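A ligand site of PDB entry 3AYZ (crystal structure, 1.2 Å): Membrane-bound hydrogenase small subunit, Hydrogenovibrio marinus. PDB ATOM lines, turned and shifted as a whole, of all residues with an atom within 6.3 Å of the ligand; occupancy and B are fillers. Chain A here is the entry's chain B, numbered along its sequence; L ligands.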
ATOM      1  N   ILE A 195     -16.139 -23.090  22.168  1.00  0.00           N
ATOM      2  CA  ILE A 195     -15.566 -22.564  23.418  1.00  0.00           C
ATOM      3  C   ILE A 195     -14.061 -22.317  23.231  1.00  0.00           C
ATOM      4  O   ILE A 195     -13.496 -21.268  23.572  1.00  0.00           O
ATOM      5  CB  ILE A 195     -15.799 -23.535  24.580  1.00  0.00           C
ATOM      6  CG1 ILE A 195     -17.228 -23.931  24.936  1.00  0.00           C
ATOM      7  CG2 ILE A 195     -15.143 -22.965  25.854  1.00  0.00           C
ATOM      8  CD1 ILE A 195     -18.117 -22.785  25.034  1.00  0.00           C
ATOM      9  N   HIS A 196     -13.339 -23.283  22.638  1.00  0.00           N
ATOM     10  CA  HIS A 196     -11.920 -23.332  22.439  1.00  0.00           C
ATOM     11  C   HIS A 196     -11.451 -22.249  21.430  1.00  0.00           C
ATOM     12  O   HIS A 196     -10.269 -21.919  21.393  1.00  0.00           O
ATOM     13  CB  HIS A 196     -11.528 -24.727  21.929  1.00  0.00           C
ATOM     14  CG  HIS A 196     -10.105 -25.091  21.698  1.00  0.00           C
ATOM     15  ND1 HIS A 196      -9.194 -25.354  22.745  1.00  0.00           N
ATOM     16  CD2 HIS A 196      -9.461 -25.319  20.536  1.00  0.00           C
ATOM     17  CE1 HIS A 196      -8.085 -25.699  22.139  1.00  0.00           C
ATOM     18  NE2 HIS A 196      -8.186 -25.657  20.841  1.00  0.00           N
ATOM     19  N   ASP A 197     -12.372 -21.765  20.589  1.00  0.00           N
ATOM     20  CA  ASP A 197     -12.090 -20.715  19.616  1.00  0.00           C
ATOM     21  C   ASP A 197     -12.039 -19.332  20.278  1.00  0.00           C
ATOM     22  O   ASP A 197     -11.707 -18.368  19.594  1.00  0.00           O
ATOM     23  CB  ASP A 197     -13.208 -20.739  18.537  1.00  0.00           C
ATOM     24  CG  ASP A 197     -13.480 -21.837  17.620  1.00  0.00           C
ATOM     25  OD1 ASP A 197     -12.424 -22.538  17.368  1.00  0.00           O
ATOM     26  OD2 ASP A 197     -14.637 -22.032  17.040  1.00  0.00           O
ATOM     27  N   CYS A 199     -11.204 -19.138  24.036  1.00  0.00           N
ATOM     28  CA  CYS A 199     -10.854 -19.494  25.412  1.00  0.00           C
ATOM     29  C   CYS A 199      -9.572 -18.782  25.873  1.00  0.00           C
ATOM     30  O   CYS A 199      -8.535 -18.979  25.231  1.00  0.00           O
ATOM     31  CB  CYS A 199     -10.680 -20.978  25.589  1.00  0.00           C
ATOM     32  SG  CYS A 199     -10.406 -21.538  27.254  1.00  0.00           S
ATOM     33  N   TYR A 200      -9.713 -18.112  26.996  1.00  0.00           N
ATOM     34  CA  TYR A 200      -8.554 -17.387  27.575  1.00  0.00           C
ATOM     35  C   TYR A 200      -7.447 -18.345  28.075  1.00  0.00           C
ATOM     36  O   TYR A 200      -6.356 -17.839  28.255  1.00  0.00           O
ATOM     37  CB  TYR A 200      -9.074 -16.446  28.706  1.00  0.00           C
ATOM     38  CG  TYR A 200      -9.210 -17.182  30.015  1.00  0.00           C
ATOM     39  CD1 TYR A 200      -8.330 -17.039  31.066  1.00  0.00           C
ATOM     40  CD2 TYR A 200     -10.226 -18.118  30.217  1.00  0.00           C
ATOM     41  CE1 TYR A 200      -8.417 -17.683  32.281  1.00  0.00           C
ATOM     42  CE2 TYR A 200     -10.318 -18.810  31.412  1.00  0.00           C
ATOM     43  CZ  TYR A 200      -9.421 -18.626  32.436  1.00  0.00           C
ATOM     44  OH  TYR A 200      -9.530 -19.398  33.574  1.00  0.00           O
ATOM     45  N   ARG A 201      -7.680 -19.623  28.228  1.00  0.00           N
ATOM     46  CA  ARG A 201      -6.643 -20.591  28.532  1.00  0.00           C
ATOM     47  C   ARG A 201      -5.887 -21.122  27.313  1.00  0.00           C
ATOM     48  O   ARG A 201      -4.944 -21.898  27.400  1.00  0.00           O
ATOM     49  CB  ARG A 201      -7.080 -21.751  29.419  1.00  0.00           C
ATOM     50  CG  ARG A 201      -7.630 -21.269  30.776  1.00  0.00           C
ATOM     51  CD  ARG A 201      -7.798 -22.460  31.725  1.00  0.00           C
ATOM     52  NE  ARG A 201      -8.354 -22.014  33.021  1.00  0.00           N
ATOM     53  CZ  ARG A 201      -8.184 -22.700  34.165  1.00  0.00           C
ATOM     54  NH1 ARG A 201      -8.763 -22.218  35.250  1.00  0.00           N
ATOM     55  NH2 ARG A 201      -7.520 -23.798  34.248  1.00  0.00           N
ATOM     56  N   ARG A 202      -6.350 -20.738  26.121  1.00  0.00           N
ATOM     57  CA  ARG A 202      -5.705 -21.154  24.883  1.00  0.00           C
ATOM     58  C   ARG A 202      -4.200 -20.931  24.809  1.00  0.00           C
ATOM     59  O   ARG A 202      -3.497 -21.827  24.291  1.00  0.00           O
ATOM     60  CB  ARG A 202      -6.366 -20.522  23.647  1.00  0.00           C
ATOM     61  CG  ARG A 202      -5.792 -20.997  22.343  1.00  0.00           C
ATOM     62  CD  ARG A 202      -6.126 -22.467  22.056  1.00  0.00           C
ATOM     63  NE  ARG A 202      -5.683 -22.722  20.671  1.00  0.00           N
ATOM     64  CZ  ARG A 202      -6.406 -22.696  19.553  1.00  0.00           C
ATOM     65  NH1 ARG A 202      -7.721 -22.497  19.627  1.00  0.00           N
ATOM     66  NH2 ARG A 202      -5.870 -22.874  18.419  1.00  0.00           N
ATOM     67  N   PRO A 203      -3.646 -19.813  25.300  1.00  0.00           N
ATOM     68  CA  PRO A 203      -2.178 -19.688  25.273  1.00  0.00           C
ATOM     69  C   PRO A 203      -1.498 -20.855  25.970  1.00  0.00           C
ATOM     70  O   PRO A 203      -0.440 -21.319  25.491  1.00  0.00           O
ATOM     71  CB  PRO A 203      -1.935 -18.423  26.074  1.00  0.00           C
ATOM     72  CG  PRO A 203      -3.213 -17.599  25.829  1.00  0.00           C
ATOM     73  CD  PRO A 203      -4.298 -18.626  25.876  1.00  0.00           C
ATOM     74  N   PHE A 205      -2.769 -24.074  26.202  1.00  0.00           N
ATOM     75  CA  PHE A 205      -2.929 -25.182  25.247  1.00  0.00           C
ATOM     76  C   PHE A 205      -1.814 -25.127  24.204  1.00  0.00           C
ATOM     77  O   PHE A 205      -1.166 -26.122  23.860  1.00  0.00           O
ATOM     78  CB  PHE A 205      -4.308 -25.075  24.593  1.00  0.00           C
ATOM     79  CG  PHE A 205      -4.603 -26.081  23.538  1.00  0.00           C
ATOM     80  CD1 PHE A 205      -4.281 -25.842  22.193  1.00  0.00           C
ATOM     81  CD2 PHE A 205      -5.183 -27.308  23.822  1.00  0.00           C
ATOM     82  CE1 PHE A 205      -4.532 -26.789  21.239  1.00  0.00           C
ATOM     83  CE2 PHE A 205      -5.448 -28.242  22.829  1.00  0.00           C
ATOM     84  CZ  PHE A 205      -5.124 -27.991  21.542  1.00  0.00           C
ATOM     85  N   PHE A 210      -0.595 -27.783  30.627  1.00  0.00           N
ATOM     86  CA  PHE A 210      -1.864 -28.442  30.997  1.00  0.00           C
ATOM     87  C   PHE A 210      -1.904 -28.732  32.448  1.00  0.00           C
ATOM     88  O   PHE A 210      -0.894 -28.995  33.163  1.00  0.00           O
ATOM     89  CB  PHE A 210      -1.956 -29.794  30.285  1.00  0.00           C
ATOM     90  CG  PHE A 210      -1.936 -29.688  28.781  1.00  0.00           C
ATOM     91  CD1 PHE A 210      -2.985 -29.110  28.093  1.00  0.00           C
ATOM     92  CD2 PHE A 210      -0.878 -30.165  28.052  1.00  0.00           C
ATOM     93  CE1 PHE A 210      -3.017 -29.010  26.764  1.00  0.00           C
ATOM     94  CE2 PHE A 210      -0.848 -30.072  26.680  1.00  0.00           C
ATOM     95  CZ  PHE A 210      -1.938 -29.475  26.017  1.00  0.00           C
ATOM     96  N   TYR A 223      -3.700 -23.356  33.877  1.00  0.00           N
ATOM     97  CA  TYR A 223      -3.293 -24.038  32.655  1.00  0.00           C
ATOM     98  C   TYR A 223      -4.476 -24.696  31.970  1.00  0.00           C
ATOM     99  O   TYR A 223      -5.573 -24.878  32.524  1.00  0.00           O
ATOM    100  CB  TYR A 223      -2.204 -25.050  32.932  1.00  0.00           C
ATOM    101  CG  TYR A 223      -0.806 -24.529  33.118  1.00  0.00           C
ATOM    102  CD1 TYR A 223      -0.508 -23.162  33.196  1.00  0.00           C
ATOM    103  CD2 TYR A 223       0.249 -25.421  33.241  1.00  0.00           C
ATOM    104  CE1 TYR A 223       0.768 -22.727  33.378  1.00  0.00           C
ATOM    105  CE2 TYR A 223       1.561 -24.968  33.401  1.00  0.00           C
ATOM    106  CZ  TYR A 223       1.835 -23.627  33.472  1.00  0.00           C
ATOM    107  OH  TYR A 223       3.133 -23.180  33.620  1.00  0.00           O
ATOM    108  N   CYS A 224      -4.338 -25.061  30.711  1.00  0.00           N
ATOM    109  CA  CYS A 224      -5.411 -25.653  29.901  1.00  0.00           C
ATOM    110  C   CYS A 224      -5.904 -26.951  30.520  1.00  0.00           C
ATOM    111  O   CYS A 224      -5.119 -27.733  31.073  1.00  0.00           O
ATOM    112  CB  CYS A 224      -4.912 -25.842  28.478  1.00  0.00           C
ATOM    113  SG  CYS A 224      -5.963 -26.792  27.395  1.00  0.00           S
ATOM    114  N   LEU A 225      -7.208 -27.166  30.364  1.00  0.00           N
ATOM    115  CA  LEU A 225      -7.939 -28.333  30.899  1.00  0.00           C
ATOM    116  C   LEU A 225      -8.137 -29.456  29.932  1.00  0.00           C
ATOM    117  O   LEU A 225      -8.835 -30.443  30.246  1.00  0.00           O
ATOM    118  CB  LEU A 225      -9.247 -27.836  31.513  1.00  0.00           C
ATOM    119  CG  LEU A 225      -9.118 -26.810  32.636  1.00  0.00           C
ATOM    120  CD1 LEU A 225     -10.441 -26.186  32.998  1.00  0.00           C
ATOM    121  CD2 LEU A 225      -8.491 -27.489  33.870  1.00  0.00           C
ATOM    122  N   TYR A 226      -7.440 -29.435  28.780  1.00  0.00           N
ATOM    123  CA  TYR A 226      -7.623 -30.462  27.761  1.00  0.00           C
ATOM    124  C   TYR A 226      -7.344 -31.850  28.336  1.00  0.00           C
ATOM    125  O   TYR A 226      -8.077 -32.816  28.050  1.00  0.00           O
ATOM    126  CB  TYR A 226      -6.687 -30.158  26.565  1.00  0.00           C
ATOM    127  CG  TYR A 226      -6.823 -31.297  25.561  1.00  0.00           C
ATOM    128  CD1 TYR A 226      -7.911 -31.371  24.710  1.00  0.00           C
ATOM    129  CD2 TYR A 226      -5.901 -32.328  25.481  1.00  0.00           C
ATOM    130  CE1 TYR A 226      -8.076 -32.392  23.819  1.00  0.00           C
ATOM    131  CE2 TYR A 226      -6.085 -33.406  24.610  1.00  0.00           C
ATOM    132  CZ  TYR A 226      -7.166 -33.406  23.764  1.00  0.00           C
ATOM    133  OH  TYR A 226      -7.291 -34.484  22.937  1.00  0.00           O
ATOM    134  N   CYS A 230     -11.522 -31.451  29.030  1.00  0.00           N
ATOM    135  CA  CYS A 230     -12.266 -30.314  28.465  1.00  0.00           C
ATOM    136  C   CYS A 230     -12.822 -30.610  27.056  1.00  0.00           C
ATOM    137  O   CYS A 230     -12.027 -30.978  26.183  1.00  0.00           O
ATOM    138  CB  CYS A 230     -11.376 -29.104  28.422  1.00  0.00           C
ATOM    139  SG  CYS A 230     -12.288 -27.607  27.942  1.00  0.00           S
ATOM    140  N   LYS A 231     -14.102 -30.423  26.868  1.00  0.00           N
ATOM    141  CA  LYS A 231     -14.784 -30.591  25.575  1.00  0.00           C
ATOM    142  C   LYS A 231     -14.973 -29.320  24.822  1.00  0.00           C
ATOM    143  O   LYS A 231     -15.645 -29.231  23.811  1.00  0.00           O
ATOM    144  CB  LYS A 231     -16.077 -31.372  25.763  1.00  0.00           C
ATOM    145  CG  LYS A 231     -15.899 -32.716  26.395  1.00  0.00           C
ATOM    146  CD  LYS A 231     -15.065 -33.659  25.646  1.00  0.00           C
ATOM    147  CE  LYS A 231     -14.383 -34.844  26.180  1.00  0.00           C
ATOM    148  NZ  LYS A 231     -14.524 -35.138  27.593  1.00  0.00           N
ATOM    149  N   GLY A 232     -14.297 -28.260  25.272  1.00  0.00           N
ATOM    150  CA  GLY A 232     -14.348 -26.978  24.575  1.00  0.00           C
ATOM    151  C   GLY A 232     -13.962 -27.077  23.149  1.00  0.00           C
ATOM    152  O   GLY A 232     -14.566 -26.331  22.295  1.00  0.00           O
ATOM    153  N   PRO A 233     -13.015 -27.898  22.706  1.00  0.00           N
ATOM    154  CA  PRO A 233     -12.666 -28.023  21.273  1.00  0.00           C
ATOM    155  C   PRO A 233     -13.802 -28.416  20.356  1.00  0.00           C
ATOM    156  O   PRO A 233     -13.694 -28.163  19.178  1.00  0.00           O
ATOM    157  CB  PRO A 233     -11.529 -29.047  21.271  1.00  0.00           C
ATOM    158  CG  PRO A 233     -10.866 -28.876  22.605  1.00  0.00           C
ATOM    159  CD  PRO A 233     -12.016 -28.665  23.522  1.00  0.00           C
ATOM    160  N   PHE A 250     -17.128 -19.105  34.034  1.00  0.00           N
ATOM    161  CA  PHE A 250     -17.665 -20.176  33.222  1.00  0.00           C
ATOM    162  C   PHE A 250     -16.911 -21.463  33.679  1.00  0.00           C
ATOM    163  O   PHE A 250     -15.969 -21.342  34.472  1.00  0.00           O
ATOM    164  CB  PHE A 250     -17.558 -19.915  31.732  1.00  0.00           C
ATOM    165  CG  PHE A 250     -16.234 -19.924  31.052  1.00  0.00           C
ATOM    166  CD1 PHE A 250     -15.863 -20.827  30.077  1.00  0.00           C
ATOM    167  CD2 PHE A 250     -15.257 -18.931  31.317  1.00  0.00           C
ATOM    168  CE1 PHE A 250     -14.720 -20.791  29.350  1.00  0.00           C
ATOM    169  CE2 PHE A 250     -14.084 -18.882  30.614  1.00  0.00           C
ATOM    170  CZ  PHE A 250     -13.778 -19.792  29.640  1.00  0.00           C
ATOM    171  N   ILE A 252     -14.611 -23.514  32.718  1.00  0.00           N
ATOM    172  CA  ILE A 252     -13.184 -23.553  32.554  1.00  0.00           C
ATOM    173  C   ILE A 252     -12.507 -22.535  33.469  1.00  0.00           C
ATOM    174  O   ILE A 252     -11.483 -22.848  34.088  1.00  0.00           O
ATOM    175  CB  ILE A 252     -12.811 -23.336  31.067  1.00  0.00           C
ATOM    176  CG1 ILE A 252     -13.207 -24.567  30.225  1.00  0.00           C
ATOM    177  CG2 ILE A 252     -11.400 -22.884  30.895  1.00  0.00           C
ATOM    178  CD1 ILE A 252     -13.685 -24.286  28.864  1.00  0.00           C
ATOM    179  N   GLY A 257     -13.048 -28.781  33.112  1.00  0.00           N
ATOM    180  CA  GLY A 257     -13.291 -28.700  31.687  1.00  0.00           C
ATOM    181  C   GLY A 257     -14.737 -28.568  31.331  1.00  0.00           C
ATOM    182  O   GLY A 257     -15.660 -29.049  32.053  1.00  0.00           O
ATOM    183  N   CYS A 258     -15.044 -27.975  30.172  1.00  0.00           N
ATOM    184  CA  CYS A 258     -16.337 -28.096  29.542  1.00  0.00           C
ATOM    185  C   CYS A 258     -16.683 -29.594  29.456  1.00  0.00           C
ATOM    186  O   CYS A 258     -15.806 -30.431  29.112  1.00  0.00           O
ATOM    187  CB  CYS A 258     -16.262 -27.462  28.175  1.00  0.00           C
ATOM    188  SG  CYS A 258     -17.670 -27.547  27.092  1.00  0.00           S
ATOM    189  N   MET A 279      -8.722 -33.460  17.165  1.00  0.00           N
ATOM    190  CA  MET A 279      -7.825 -32.342  17.469  1.00  0.00           C
ATOM    191  C   MET A 279      -6.847 -32.062  16.334  1.00  0.00           C
ATOM    192  O   MET A 279      -6.557 -30.886  16.005  1.00  0.00           O
ATOM    193  CB  MET A 279      -7.128 -32.623  18.803  1.00  0.00           C
ATOM    194  CG  MET A 279      -8.127 -32.767  19.965  1.00  0.00           C
ATOM    195  SD  MET A 279      -9.124 -31.431  20.413  1.00  0.00           S
ATOM    196  CE  MET A 279      -7.880 -30.139  20.797  1.00  0.00           C
HETATM  197 FE1  LIG L   1      -9.771 -23.688  26.869  1.00  0.00          FE
HETATM  198 FE2  LIG L   1      -7.931 -25.707  26.950  1.00  0.00          FE
HETATM  199 FE3  LIG L   1     -10.619 -26.277  27.070  1.00  0.00          FE
HETATM  200 FE4  LIG L   1      -9.489 -25.359  24.776  1.00  0.00          FE
HETATM  201  S1  LIG L   1      -9.101 -27.352  25.795  1.00  0.00           S
HETATM  202  S2  LIG L   1     -11.457 -24.707  25.650  1.00  0.00           S
HETATM  203  S3  LIG L   1      -7.899 -23.893  25.580  1.00  0.00           S
HETATM  204  S4  LIG L   1      -9.335 -25.100  28.626  1.00  0.00           S
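An iron atom (FE4) of the ligand is bound by a ring nitrogen (ND1) of His 196. An iron atom (FE1) of the ligand is bound by the side-chain sulfur (SG) of Cys 199 (2.3 Å). An iron atom (FE2) of the ligand is bound by the side-chain sulfur (SG) of Cys 224, at 2.3 Å. FE3 of the ligand is bound by SG of Cys 230, 2.3 Å away. N of Leu 225 lies close to S4 of the ligand (3.4 Å). N of Arg 202 lies close to S3 of the ligand.
The backbone carbonyl oxygen (O) of His 196 lies within hydrogen-bond range of the guanidinium group (NH1) of Arg 202, 3.2 Å away. N of His 196 sits at hydrogen-bond distance from O of Gly 232 (3.3 Å). N of Tyr 226 sits close to SG of Cys 224, 3.3 Å away. The backbone carbonyl oxygen (O) of Leu 225 lies within hydrogen-bond range of the backbone NH (N) of Cys 230 (3.1 Å). The side-chain sulfur of Cys 230 sits close to the backbone NH of Gly 232, at 3.4 Å. NH1 of Arg 201 lies within hydrogen-bond range of O of Ile 252. The guanidinium group (NH2) of Arg 201 sits at hydrogen-bond distance from the backbone carbonyl oxygen (O) of Tyr 223, 2.8 Å away. OH of Tyr 200 is in hydrogen-bond range of NE of Arg 201 (2.9 Å).
Arg 201 touches the ligand (C to S3, 3.8 Å). Phe 205 touches the ligand. Tyr 226 touches the ligand. CA of Gly 232 touches S2 of the ligand (3.8 Å). Pro 233 touches the ligand (CD to S1, 3.9 Å). CG2 of Ile 252 touches S4 of the ligand, 3.8 Å away. Hydrophobic or aromatic side chains that line the ligand: His 196, Phe 205, Leu 225, Tyr 226, Pro 233 and Ile 252. 12 residues have an atom within 4 Å of the ligand: His 196, Cys 199, Arg 201, Arg 202, Phe 205, Cys 224, Leu 225, Tyr 226, Cys 230, Gly 232, Pro 233 and Ile 252.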
